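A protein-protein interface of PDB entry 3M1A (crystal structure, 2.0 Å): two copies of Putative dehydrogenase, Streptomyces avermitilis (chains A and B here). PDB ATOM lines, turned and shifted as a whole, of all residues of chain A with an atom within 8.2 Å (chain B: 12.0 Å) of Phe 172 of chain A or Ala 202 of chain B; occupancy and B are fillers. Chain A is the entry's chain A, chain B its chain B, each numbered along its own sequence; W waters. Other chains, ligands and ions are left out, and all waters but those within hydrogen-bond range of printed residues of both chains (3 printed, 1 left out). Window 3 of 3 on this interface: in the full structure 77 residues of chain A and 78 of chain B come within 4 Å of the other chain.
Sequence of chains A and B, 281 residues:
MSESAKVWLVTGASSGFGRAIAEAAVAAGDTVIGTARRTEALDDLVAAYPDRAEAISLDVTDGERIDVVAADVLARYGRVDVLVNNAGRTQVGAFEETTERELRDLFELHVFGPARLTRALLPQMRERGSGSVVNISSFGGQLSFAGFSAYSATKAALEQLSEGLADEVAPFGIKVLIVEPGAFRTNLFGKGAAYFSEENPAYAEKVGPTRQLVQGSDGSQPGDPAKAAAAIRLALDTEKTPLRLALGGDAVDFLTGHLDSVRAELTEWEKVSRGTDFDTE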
ATOM      1  N   LEU A 122       0.007  17.422  -3.164  1.00  0.00           N
ATOM      2  CA  LEU A 122       0.505  18.762  -3.418  1.00  0.00           C
ATOM      3  C   LEU A 122       1.771  18.775  -4.276  1.00  0.00           C
ATOM      4  O   LEU A 122       1.849  19.585  -5.164  1.00  0.00           O
ATOM      5  CB  LEU A 122       0.726  19.514  -2.086  1.00  0.00           C
ATOM      6  CG  LEU A 122      -0.090  20.724  -1.608  1.00  0.00           C
ATOM      7  CD1 LEU A 122      -1.430  20.989  -2.279  1.00  0.00           C
ATOM      8  CD2 LEU A 122      -0.233  20.723  -0.084  1.00  0.00           C
ATOM      9  N   PRO A 123       2.779  17.901  -3.985  1.00  0.00           N
ATOM     10  CA  PRO A 123       4.017  18.010  -4.773  1.00  0.00           C
ATOM     11  C   PRO A 123       3.749  18.015  -6.302  1.00  0.00           C
ATOM     12  O   PRO A 123       4.240  18.929  -6.990  1.00  0.00           O
ATOM     13  CB  PRO A 123       4.826  16.751  -4.350  1.00  0.00           C
ATOM     14  CG  PRO A 123       4.463  16.587  -2.865  1.00  0.00           C
ATOM     15  CD  PRO A 123       2.927  16.952  -2.862  1.00  0.00           C
ATOM     16  N   MET A 125       1.064  18.809  -7.958  1.00  0.00           N
ATOM     17  CA  MET A 125       0.420  20.062  -8.370  1.00  0.00           C
ATOM     18  C   MET A 125       1.445  21.191  -8.490  1.00  0.00           C
ATOM     19  O   MET A 125       1.358  22.015  -9.409  1.00  0.00           O
ATOM     20  CB  MET A 125      -0.674  20.494  -7.389  1.00  0.00           C
ATOM     21  CG  MET A 125      -1.821  19.506  -7.264  1.00  0.00           C
ATOM     22  SD  MET A 125      -3.186  20.210  -6.052  1.00  0.00           S
ATOM     23  CE  MET A 125      -4.514  18.710  -6.275  1.00  0.00           C
ATOM     24  N   ARG A 126       2.384  21.251  -7.541  1.00  0.00           N
ATOM     25  CA  ARG A 126       3.445  22.279  -7.578  1.00  0.00           C
ATOM     26  C   ARG A 126       4.306  22.095  -8.805  1.00  0.00           C
ATOM     27  O   ARG A 126       4.626  23.071  -9.497  1.00  0.00           O
ATOM     28  CB  ARG A 126       4.354  22.211  -6.341  1.00  0.00           C
ATOM     29  CG  ARG A 126       3.799  22.889  -5.099  1.00  0.00           C
ATOM     30  CD  ARG A 126       4.926  23.041  -4.050  1.00  0.00           C
ATOM     31  NE  ARG A 126       5.179  21.810  -3.285  1.00  0.00           N
ATOM     32  CZ  ARG A 126       6.134  20.890  -3.530  1.00  0.00           C
ATOM     33  NH1 ARG A 126       6.276  19.832  -2.714  1.00  0.00           N
ATOM     34  NH2 ARG A 126       6.950  21.007  -4.572  1.00  0.00           N
ATOM     35  N   GLU A 127       4.672  20.831  -9.061  1.00  0.00           N
ATOM     36  CA  GLU A 127       5.486  20.436 -10.202  1.00  0.00           C
ATOM     37  C   GLU A 127       4.849  20.848 -11.533  1.00  0.00           C
ATOM     38  O   GLU A 127       5.542  21.303 -12.449  1.00  0.00           O
ATOM     39  CB  GLU A 127       5.768  18.927 -10.176  1.00  0.00           C
ATOM     40  CG  GLU A 127       6.834  18.542  -9.164  1.00  0.00           C
ATOM     41  CD  GLU A 127       6.915  17.039  -8.872  1.00  0.00           C
ATOM     42  OE1 GLU A 127       6.726  16.207  -9.795  1.00  0.00           O
ATOM     43  OE2 GLU A 127       7.186  16.703  -7.700  1.00  0.00           O
ATOM     44  N   ARG A 128       3.543  20.663 -11.632  1.00  0.00           N
ATOM     45  CA  ARG A 128       2.797  21.059 -12.808  1.00  0.00           C
ATOM     46  C   ARG A 128       2.671  22.576 -12.850  1.00  0.00           C
ATOM     47  O   ARG A 128       2.736  23.186 -13.919  1.00  0.00           O
ATOM     48  CB  ARG A 128       1.402  20.440 -12.758  1.00  0.00           C
ATOM     49  CG  ARG A 128       0.579  20.635 -14.018  1.00  0.00           C
ATOM     50  CD  ARG A 128      -0.633  19.696 -14.039  1.00  0.00           C
ATOM     51  NE  ARG A 128      -1.373  19.703 -12.774  1.00  0.00           N
ATOM     52  CZ  ARG A 128      -1.455  18.668 -11.940  1.00  0.00           C
ATOM     53  NH1 ARG A 128      -2.152  18.771 -10.819  1.00  0.00           N
ATOM     54  NH2 ARG A 128      -0.842  17.534 -12.226  1.00  0.00           N
ATOM     55  N   GLY A 129       2.496  23.181 -11.681  1.00  0.00           N
ATOM     56  CA  GLY A 129       2.102  24.581 -11.608  1.00  0.00           C
ATOM     57  C   GLY A 129       0.590  24.762 -11.773  1.00  0.00           C
ATOM     58  O   GLY A 129       0.128  25.851 -12.098  1.00  0.00           O
ATOM     59  N   SER A 130      -0.187  23.706 -11.563  1.00  0.00           N
ATOM     60  CA  SER A 130      -1.660  23.858 -11.480  1.00  0.00           C
ATOM     61  C   SER A 130      -2.292  22.770 -10.636  1.00  0.00           C
ATOM     62  O   SER A 130      -1.693  21.708 -10.453  1.00  0.00           O
ATOM     63  CB  SER A 130      -2.316  23.851 -12.869  1.00  0.00           C
ATOM     64  OG  SER A 130      -2.059  22.618 -13.516  1.00  0.00           O
ATOM     65  N   GLY A 131      -3.517  23.032 -10.160  1.00  0.00           N
ATOM     66  CA  GLY A 131      -4.307  22.090  -9.378  1.00  0.00           C
ATOM     67  C   GLY A 131      -5.317  22.798  -8.476  1.00  0.00           C
ATOM     68  O   GLY A 131      -5.190  24.001  -8.209  1.00  0.00           O
ATOM     69  N   LEU A 165      -3.048  27.249   3.906  1.00  0.00           N
ATOM     70  CA  LEU A 165      -2.556  26.629   2.669  1.00  0.00           C
ATOM     71  C   LEU A 165      -2.794  27.518   1.452  1.00  0.00           C
ATOM     72  O   LEU A 165      -1.876  27.735   0.669  1.00  0.00           O
ATOM     73  CB  LEU A 165      -3.210  25.247   2.444  1.00  0.00           C
ATOM     74  CG  LEU A 165      -2.934  24.521   1.127  1.00  0.00           C
ATOM     75  CD1 LEU A 165      -1.450  24.124   1.054  1.00  0.00           C
ATOM     76  CD2 LEU A 165      -3.830  23.311   1.023  1.00  0.00           C
ATOM     77  N   ALA A 166      -4.008  28.059   1.310  1.00  0.00           N
ATOM     78  CA  ALA A 166      -4.349  28.902   0.142  1.00  0.00           C
ATOM     79  C   ALA A 166      -3.354  30.037  -0.066  1.00  0.00           C
ATOM     80  O   ALA A 166      -2.957  30.339  -1.201  1.00  0.00           O
ATOM     81  CB  ALA A 166      -5.724  29.484   0.287  1.00  0.00           C
ATOM     82  N   ASP A 167      -2.992  30.678   1.049  1.00  0.00           N
ATOM     83  CA  ASP A 167      -2.114  31.846   1.055  1.00  0.00           C
ATOM     84  C   ASP A 167      -0.708  31.395   0.594  1.00  0.00           C
ATOM     85  O   ASP A 167       0.012  32.145  -0.067  1.00  0.00           O
ATOM     86  CB  ASP A 167      -2.091  32.464   2.472  1.00  0.00           C
ATOM     87  CG  ASP A 167      -1.482  33.858   2.510  1.00  0.00           C
ATOM     88  OD1 ASP A 167      -1.751  34.654   1.581  1.00  0.00           O
ATOM     89  OD2 ASP A 167      -0.723  34.164   3.468  1.00  0.00           O
ATOM     90  N   GLU A 168      -0.353  30.162   0.906  1.00  0.00           N
ATOM     91  CA  GLU A 168       0.991  29.640   0.570  1.00  0.00           C
ATOM     92  C   GLU A 168       1.171  29.175  -0.884  1.00  0.00           C
ATOM     93  O   GLU A 168       2.263  29.326  -1.453  1.00  0.00           O
ATOM     94  CB  GLU A 168       1.374  28.497   1.498  1.00  0.00           C
ATOM     95  CG  GLU A 168       1.529  28.915   2.951  1.00  0.00           C
ATOM     96  CD  GLU A 168       1.590  27.755   3.923  1.00  0.00           C
ATOM     97  OE1 GLU A 168       1.567  26.594   3.470  1.00  0.00           O
ATOM     98  OE2 GLU A 168       1.655  28.016   5.144  1.00  0.00           O
ATOM     99  N   VAL A 169       0.124  28.589  -1.452  1.00  0.00           N
ATOM    100  CA  VAL A 169       0.214  27.927  -2.742  1.00  0.00           C
ATOM    101  C   VAL A 169      -0.325  28.736  -3.912  1.00  0.00           C
ATOM    102  O   VAL A 169      -0.177  28.333  -5.067  1.00  0.00           O
ATOM    103  CB  VAL A 169      -0.382  26.481  -2.722  1.00  0.00           C
ATOM    104  CG1 VAL A 169       0.366  25.630  -1.690  1.00  0.00           C
ATOM    105  CG2 VAL A 169      -1.879  26.479  -2.464  1.00  0.00           C
ATOM    106  N   ALA A 170      -0.925  29.882  -3.621  1.00  0.00           N
ATOM    107  CA  ALA A 170      -1.314  30.811  -4.680  1.00  0.00           C
ATOM    108  C   ALA A 170      -0.166  31.101  -5.683  1.00  0.00           C
ATOM    109  O   ALA A 170      -0.402  31.067  -6.890  1.00  0.00           O
ATOM    110  CB  ALA A 170      -1.907  32.114  -4.094  1.00  0.00           C
ATOM    111  N   PRO A 171       1.070  31.364  -5.198  1.00  0.00           N
ATOM    112  CA  PRO A 171       2.186  31.566  -6.138  1.00  0.00           C
ATOM    113  C   PRO A 171       2.509  30.365  -7.041  1.00  0.00           C
ATOM    114  O   PRO A 171       3.164  30.533  -8.055  1.00  0.00           O
ATOM    115  CB  PRO A 171       3.385  31.845  -5.214  1.00  0.00           C
ATOM    116  CG  PRO A 171       2.781  32.374  -3.972  1.00  0.00           C
ATOM    117  CD  PRO A 171       1.485  31.639  -3.808  1.00  0.00           C
ATOM    118  N   PHE A 172       2.074  29.169  -6.659  1.00  0.00           N
ATOM    119  CA  PHE A 172       2.336  27.973  -7.456  1.00  0.00           C
ATOM    120  C   PHE A 172       1.245  27.710  -8.517  1.00  0.00           C
ATOM    121  O   PHE A 172       1.348  26.760  -9.288  1.00  0.00           O
ATOM    122  CB  PHE A 172       2.502  26.740  -6.556  1.00  0.00           C
ATOM    123  CG  PHE A 172       3.529  26.900  -5.442  1.00  0.00           C
ATOM    124  CD1 PHE A 172       3.215  26.508  -4.140  1.00  0.00           C
ATOM    125  CD2 PHE A 172       4.798  27.402  -5.691  1.00  0.00           C
ATOM    126  CE1 PHE A 172       4.145  26.613  -3.103  1.00  0.00           C
ATOM    127  CE2 PHE A 172       5.734  27.529  -4.654  1.00  0.00           C
ATOM    128  CZ  PHE A 172       5.403  27.135  -3.362  1.00  0.00           C
ATOM    129  N   GLY A 173       0.217  28.555  -8.547  1.00  0.00           N
ATOM    130  CA  GLY A 173      -0.935  28.396  -9.455  1.00  0.00           C
ATOM    131  C   GLY A 173      -1.938  27.372  -8.941  1.00  0.00           C
ATOM    132  O   GLY A 173      -2.781  26.885  -9.698  1.00  0.00           O
ATOM    133  N   ILE A 174      -1.851  27.038  -7.655  1.00  0.00           N
ATOM    134  CA  ILE A 174      -2.775  26.084  -7.029  1.00  0.00           C
ATOM    135  C   ILE A 174      -3.968  26.812  -6.386  1.00  0.00           C
ATOM    136  O   ILE A 174      -3.789  27.797  -5.661  1.00  0.00           O
ATOM    137  CB  ILE A 174      -2.033  25.205  -5.997  1.00  0.00           C
ATOM    138  CG1 ILE A 174      -0.872  24.456  -6.694  1.00  0.00           C
ATOM    139  CG2 ILE A 174      -3.004  24.231  -5.249  1.00  0.00           C
ATOM    140  CD1 ILE A 174       0.022  23.669  -5.766  1.00  0.00           C
ATOM    141  N   LYS A 175      -5.165  26.320  -6.667  1.00  0.00           N
ATOM    142  CA  LYS A 175      -6.405  26.868  -6.096  1.00  0.00           C
ATOM    143  C   LYS A 175      -6.860  26.092  -4.865  1.00  0.00           C
ATOM    144  O   LYS A 175      -6.781  24.866  -4.818  1.00  0.00           O
ATOM    145  CB  LYS A 175      -7.528  26.849  -7.138  1.00  0.00           C
ATOM    146  CG  LYS A 175      -7.402  27.829  -8.306  1.00  0.00           C
ATOM    147  CD  LYS A 175      -8.364  27.389  -9.414  1.00  0.00           C
ATOM    148  CE  LYS A 175      -8.162  28.087 -10.757  1.00  0.00           C
ATOM    149  NZ  LYS A 175      -8.536  29.499 -10.736  1.00  0.00           N
ATOM    150  N   GLY B  93       5.207  27.323  10.201  1.00  0.00           N
ATOM    151  CA  GLY B  93       5.835  26.598   9.111  1.00  0.00           C
ATOM    152  C   GLY B  93       4.808  26.348   8.039  1.00  0.00           C
ATOM    153  O   GLY B  93       3.593  26.323   8.339  1.00  0.00           O
ATOM    154  N   ALA B  94       5.291  26.212   6.799  1.00  0.00           N
ATOM    155  CA  ALA B  94       4.456  25.910   5.641  1.00  0.00           C
ATOM    156  C   ALA B  94       3.660  24.650   5.909  1.00  0.00           C
ATOM    157  O   ALA B  94       4.147  23.718   6.567  1.00  0.00           O
ATOM    158  CB  ALA B  94       5.301  25.714   4.386  1.00  0.00           C
ATOM    159  N   PHE B  95       2.431  24.637   5.403  1.00  0.00           N
ATOM    160  CA  PHE B  95       1.575  23.449   5.495  1.00  0.00           C
ATOM    161  C   PHE B  95       2.340  22.147   5.141  1.00  0.00           C
ATOM    162  O   PHE B  95       2.288  21.190   5.902  1.00  0.00           O
ATOM    163  CB  PHE B  95       0.329  23.648   4.623  1.00  0.00           C
ATOM    164  CG  PHE B  95      -0.578  22.452   4.556  1.00  0.00           C
ATOM    165  CD1 PHE B  95      -0.367  21.456   3.593  1.00  0.00           C
ATOM    166  CD2 PHE B  95      -1.660  22.335   5.420  1.00  0.00           C
ATOM    167  CE1 PHE B  95      -1.223  20.334   3.512  1.00  0.00           C
ATOM    168  CE2 PHE B  95      -2.524  21.226   5.345  1.00  0.00           C
ATOM    169  CZ  PHE B  95      -2.304  20.227   4.401  1.00  0.00           C
ATOM    170  N   GLU B  96       3.052  22.126   4.011  1.00  0.00           N
ATOM    171  CA  GLU B  96       3.815  20.937   3.597  1.00  0.00           C
ATOM    172  C   GLU B  96       4.996  20.609   4.505  1.00  0.00           C
ATOM    173  O   GLU B  96       5.442  19.458   4.538  1.00  0.00           O
ATOM    174  CB  GLU B  96       4.339  21.084   2.173  1.00  0.00           C
ATOM    175  CG  GLU B  96       3.312  20.892   1.108  1.00  0.00           C
ATOM    176  CD  GLU B  96       3.938  20.800  -0.253  1.00  0.00           C
ATOM    177  OE1 GLU B  96       4.252  21.866  -0.825  1.00  0.00           O
ATOM    178  OE2 GLU B  96       4.141  19.671  -0.743  1.00  0.00           O
ATOM    179  N   GLU B  97       5.533  21.606   5.198  1.00  0.00           N
ATOM    180  CA  GLU B  97       6.637  21.365   6.142  1.00  0.00           C
ATOM    181  C   GLU B  97       6.181  20.733   7.476  1.00  0.00           C
ATOM    182  O   GLU B  97       6.986  20.092   8.162  1.00  0.00           O
ATOM    183  CB  GLU B  97       7.369  22.675   6.444  1.00  0.00           C
ATOM    184  CG  GLU B  97       8.192  23.201   5.294  1.00  0.00           C
ATOM    185  CD  GLU B  97       9.383  22.299   4.977  1.00  0.00           C
ATOM    186  OE1 GLU B  97       9.851  21.544   5.867  1.00  0.00           O
ATOM    187  OE2 GLU B  97       9.857  22.360   3.835  1.00  0.00           O
ATOM    188  N   ALA B 146      -0.121  32.382   5.570  1.00  0.00           N
ATOM    189  CA  ALA B 146       1.044  31.524   5.337  1.00  0.00           C
ATOM    190  C   ALA B 146       1.829  31.307   6.630  1.00  0.00           C
ATOM    191  O   ALA B 146       2.043  32.270   7.386  1.00  0.00           O
ATOM    192  CB  ALA B 146       1.933  32.120   4.261  1.00  0.00           C
ATOM    193  N   GLY B 147       2.210  30.053   6.891  1.00  0.00           N
ATOM    194  CA  GLY B 147       3.039  29.699   8.046  1.00  0.00           C
ATOM    195  C   GLY B 147       2.265  29.380   9.321  1.00  0.00           C
ATOM    196  O   GLY B 147       2.835  28.872  10.280  1.00  0.00           O
ATOM    197  N   SER B 197       9.577  25.932  11.378  1.00  0.00           N
ATOM    198  CA  SER B 197      10.069  25.025  10.341  1.00  0.00           C
ATOM    199  C   SER B 197      11.061  25.737   9.435  1.00  0.00           C
ATOM    200  O   SER B 197      11.046  26.980   9.312  1.00  0.00           O
ATOM    201  CB  SER B 197       8.906  24.508   9.483  1.00  0.00           C
ATOM    202  OG  SER B 197       7.912  23.876  10.274  1.00  0.00           O
ATOM    203  N   GLU B 198      11.922  24.940   8.808  1.00  0.00           N
ATOM    204  CA  GLU B 198      12.722  25.358   7.666  1.00  0.00           C
ATOM    205  C   GLU B 198      11.867  26.179   6.686  1.00  0.00           C
ATOM    206  O   GLU B 198      10.702  25.862   6.428  1.00  0.00           O
ATOM    207  CB  GLU B 198      13.288  24.118   6.984  1.00  0.00           C
ATOM    208  CG  GLU B 198      14.266  24.385   5.890  1.00  0.00           C
ATOM    209  CD  GLU B 198      14.878  23.102   5.344  1.00  0.00           C
ATOM    210  OE1 GLU B 198      14.500  22.710   4.228  1.00  0.00           O
ATOM    211  OE2 GLU B 198      15.726  22.492   6.030  1.00  0.00           O
ATOM    212  N   GLU B 199      12.462  27.257   6.195  1.00  0.00           N
ATOM    213  CA  GLU B 199      11.812  28.235   5.357  1.00  0.00           C
ATOM    214  C   GLU B 199      12.596  28.394   4.036  1.00  0.00           C
ATOM    215  O   GLU B 199      13.479  29.258   3.923  1.00  0.00           O
ATOM    216  CB  GLU B 199      11.799  29.551   6.116  1.00  0.00           C
ATOM    217  CG  GLU B 199      10.538  30.336   6.008  1.00  0.00           C
ATOM    218  CD  GLU B 199      10.436  31.402   7.092  1.00  0.00           C
ATOM    219  OE1 GLU B 199      10.272  31.049   8.305  1.00  0.00           O
ATOM    220  OE2 GLU B 199      10.501  32.593   6.709  1.00  0.00           O
ATOM    221  N   ASN B 200      12.264  27.565   3.046  1.00  0.00           N
ATOM    222  CA  ASN B 200      12.964  27.589   1.759  1.00  0.00           C
ATOM    223  C   ASN B 200      12.532  28.753   0.853  1.00  0.00           C
ATOM    224  O   ASN B 200      11.416  29.279   0.995  1.00  0.00           O
ATOM    225  CB  ASN B 200      12.933  26.216   1.049  1.00  0.00           C
ATOM    226  CG  ASN B 200      11.537  25.786   0.591  1.00  0.00           C
ATOM    227  OD1 ASN B 200      11.303  24.602   0.341  1.00  0.00           O
ATOM    228  ND2 ASN B 200      10.618  26.735   0.465  1.00  0.00           N
ATOM    229  N   PRO B 201      13.425  29.183  -0.072  1.00  0.00           N
ATOM    230  CA  PRO B 201      13.118  30.341  -0.918  1.00  0.00           C
ATOM    231  C   PRO B 201      11.724  30.333  -1.550  1.00  0.00           C
ATOM    232  O   PRO B 201      11.162  31.401  -1.792  1.00  0.00           O
ATOM    233  CB  PRO B 201      14.182  30.261  -2.011  1.00  0.00           C
ATOM    234  CG  PRO B 201      15.325  29.655  -1.358  1.00  0.00           C
ATOM    235  CD  PRO B 201      14.788  28.678  -0.351  1.00  0.00           C
ATOM    236  N   ALA B 202      11.167  29.148  -1.794  1.00  0.00           N
ATOM    237  CA  ALA B 202       9.864  29.034  -2.444  1.00  0.00           C
ATOM    238  C   ALA B 202       8.714  29.484  -1.543  1.00  0.00           C
ATOM    239  O   ALA B 202       7.629  29.824  -2.030  1.00  0.00           O
ATOM    240  CB  ALA B 202       9.642  27.608  -2.940  1.00  0.00           C
ATOM    241  N   TYR B 203       8.950  29.480  -0.235  1.00  0.00           N
ATOM    242  CA  TYR B 203       7.940  29.837   0.745  1.00  0.00           C
ATOM    243  C   TYR B 203       8.350  31.072   1.578  1.00  0.00           C
ATOM    244  O   TYR B 203       7.563  31.566   2.408  1.00  0.00           O
ATOM    245  CB  TYR B 203       7.671  28.636   1.679  1.00  0.00           C
ATOM    246  CG  TYR B 203       6.747  27.541   1.152  1.00  0.00           C
ATOM    247  CD1 TYR B 203       5.445  27.828   0.768  1.00  0.00           C
ATOM    248  CD2 TYR B 203       7.159  26.203   1.092  1.00  0.00           C
ATOM    249  CE1 TYR B 203       4.580  26.832   0.307  1.00  0.00           C
ATOM    250  CE2 TYR B 203       6.280  25.177   0.612  1.00  0.00           C
ATOM    251  CZ  TYR B 203       4.984  25.507   0.221  1.00  0.00           C
ATOM    252  OH  TYR B 203       4.059  24.547  -0.261  1.00  0.00           O
ATOM    253  N   ALA B 204       9.568  31.568   1.370  1.00  0.00           N
ATOM    254  CA  ALA B 204      10.111  32.599   2.253  1.00  0.00           C
ATOM    255  C   ALA B 204       9.334  33.919   2.215  1.00  0.00           C
ATOM    256  O   ALA B 204       9.079  34.501   3.264  1.00  0.00           O
ATOM    257  CB  ALA B 204      11.612  32.816   2.022  1.00  0.00           C
ATOM    258  N   GLU B 205       8.941  34.371   1.027  1.00  0.00           N
ATOM    259  CA  GLU B 205       8.174  35.617   0.859  1.00  0.00           C
ATOM    260  C   GLU B 205       6.843  35.630   1.638  1.00  0.00           C
ATOM    261  O   GLU B 205       6.432  36.663   2.177  1.00  0.00           O
ATOM    262  CB  GLU B 205       7.921  35.901  -0.643  1.00  0.00           C
ATOM    263  N   LYS B 206       6.179  34.475   1.686  1.00  0.00           N
ATOM    264  CA  LYS B 206       4.917  34.316   2.384  1.00  0.00           C
ATOM    265  C   LYS B 206       5.081  33.958   3.862  1.00  0.00           C
ATOM    266  O   LYS B 206       4.392  34.503   4.733  1.00  0.00           O
ATOM    267  CB  LYS B 206       4.080  33.244   1.688  1.00  0.00           C
ATOM    268  CG  LYS B 206       3.464  33.715   0.384  1.00  0.00           C
ATOM    269  CD  LYS B 206       2.333  34.671   0.673  1.00  0.00           C
ATOM    270  CE  LYS B 206       1.787  35.249  -0.599  1.00  0.00           C
ATOM    271  NZ  LYS B 206       0.372  35.651  -0.329  1.00  0.00           N
ATOM    272  N   VAL B 207       5.981  33.031   4.157  1.00  0.00           N
ATOM    273  CA  VAL B 207       6.100  32.555   5.532  1.00  0.00           C
ATOM    274  C   VAL B 207       6.947  33.497   6.377  1.00  0.00           C
ATOM    275  O   VAL B 207       6.662  33.703   7.553  1.00  0.00           O
ATOM    276  CB  VAL B 207       6.548  31.080   5.585  1.00  0.00           C
ATOM    277  CG1 VAL B 207       6.749  30.608   7.014  1.00  0.00           C
ATOM    278  CG2 VAL B 207       5.514  30.214   4.889  1.00  0.00           C
ATOM    279  N   GLY B 208       7.975  34.082   5.766  1.00  0.00           N
ATOM    280  CA  GLY B 208       8.901  34.989   6.463  1.00  0.00           C
ATOM    281  C   GLY B 208       8.237  35.998   7.383  1.00  0.00           C
ATOM    282  O   GLY B 208       8.590  36.078   8.556  1.00  0.00           O
ATOM    283  N   PRO B 209       7.275  36.777   6.853  1.00  0.00           N
ATOM    284  CA  PRO B 209       6.502  37.750   7.638  1.00  0.00           C
ATOM    285  C   PRO B 209       5.779  37.175   8.855  1.00  0.00           C
ATOM    286  O   PRO B 209       5.627  37.868   9.859  1.00  0.00           O
ATOM    287  CB  PRO B 209       5.493  38.279   6.616  1.00  0.00           C
ATOM    288  CG  PRO B 209       6.263  38.229   5.318  1.00  0.00           C
ATOM    289  CD  PRO B 209       7.049  36.953   5.401  1.00  0.00           C
ATOM    290  N   ARG B 211       6.805  34.449  10.662  1.00  0.00           N
ATOM    291  CA  ARG B 211       7.887  34.233  11.643  1.00  0.00           C
ATOM    292  C   ARG B 211       8.265  35.519  12.378  1.00  0.00           C
ATOM    293  O   ARG B 211       8.476  35.520  13.612  1.00  0.00           O
ATOM    294  CB  ARG B 211       9.141  33.677  10.948  1.00  0.00           C
ATOM    295  CG  ARG B 211      10.316  33.395  11.888  1.00  0.00           C
ATOM    296  CD  ARG B 211      11.571  32.861  11.171  1.00  0.00           C
ATOM    297  NE  ARG B 211      11.652  33.306   9.786  1.00  0.00           N
ATOM    298  CZ  ARG B 211      12.381  34.323   9.347  1.00  0.00           C
ATOM    299  NH1 ARG B 211      12.351  34.621   8.055  1.00  0.00           N
ATOM    300  NH2 ARG B 211      13.141  35.034  10.171  1.00  0.00           N
HETATM  301  O   HOH W   1       2.627  24.371   2.094  1.00  0.00           O
HETATM  302  O   HOH W   2       1.113  26.819   7.350  1.00  0.00           O
HETATM  303  O   HOH W   3       4.726  30.555  -1.047  1.00  0.00           O
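The side-chain carboxylate of Glu 168 of chain A is in hydrogen-bond range of the backbone NH of Gly 147 of chain B (2.7 Å). The side-chain carboxylate (OE1) of Glu 96 of chain B lies within salt-bridge range of the guanidinium group (NE) of Arg 126 of chain A (2.6 Å). The side-chain carboxylate (OD2) of Asp 167 of chain A sits at hydrogen-bond distance from the backbone NH (N) of Ala 146 of chain B (2.8 Å). OD1 of Asp 167 of chain A is in salt-bridge range of NZ of Lys 206 of chain B (3.0 Å). The side-chain carboxylate (OE1) of Glu 168 of chain A lies within hydrogen-bond range of the backbone NH (N) of Phe 95 of chain B (2.9 Å).
The side-chain amide nitrogen of Asn 200 of chain B sits close to the backbone NH of Tyr 203 of chain B (3.3 Å). ND2 of Asn 200 of chain B sits close to N of Ala 202 of chain B. OE1 of Glu 96 of chain B is in hydrogen-bond range of OH of Tyr 203 of chain B (2.7 Å).
Among the printed residues, pairs that only touch across the chains: Leu 122 of chain A with Phe 95 of chain B (3.8 Å), Leu 122 of chain A with Glu 96 of chain B (3.7 Å), Pro 123 of chain A with Glu 96 of chain B (3.7 Å), Leu 165 of chain A with Phe 95 of chain B (3.8 Å), Glu 168 of chain A with Ala 94 of chain B (3.5 Å), Glu 168 of chain A with Ala 146 of chain B (3.5 Å), Glu 168 of chain A with Tyr 203 of chain B (3.8 Å), Phe 172 of chain A with Ala 202 of chain B (3.7 Å) and Phe 172 of chain A with Tyr 203 of chain B (3.4 Å).
Arg 126 of chain A touches just one residue of chain B: Glu 96 (2.6 Å). No residue of chain B comes within 4 Å of Ser 130 of chain A. Gly 131 of chain A touches none of the printed residues of chain B. Of the printed residues of chain B, Asp 167 of chain A touches Ala 146 and Lys 206. No residue of chain B comes within 4 Å of Val 169 of chain A. Ala 170 of chain A touches none of the printed residues of chain B. No residue of chain B comes within 4 Å of Ile 174 of chain A. The nearest residue of chain A that does not touch Ala 202 of chain B is Glu 168 of chain A (5.4 Å). The nearest printed residue of chain B that does not touch Glu 168 of chain A is Gly 93 of chain B (4.1 Å).
Printed residues of chain B that touch a printed residue of chain A: Ala 94, Phe 95, Glu 96, Ala 146, Gly 147, Ala 202, Tyr 203 and Lys 206. Among the printed residues, Asp or Glu carboxylates within 4 Å of a Lys or Arg side-chain nitrogen of the other chain: Arg 126 of chain A with Glu 96 of chain B (2.6 Å) and Asp 167 of chain A with Lys 206 of chain B (3.0 Å).
No position is printed for both chains. Of the 14 pairs that touch across the chains among the printed residues, none has its exchanged pair printed and touching as well.
Water W1 lies within hydrogen-bond range of OH of Tyr 203 of chain B (2.8 Å), OE1 of Glu 168 of chain A (2.8 Å), N of Glu 96 of chain B (3.0 Å) and N of Phe 95 of chain B (3.3 Å).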
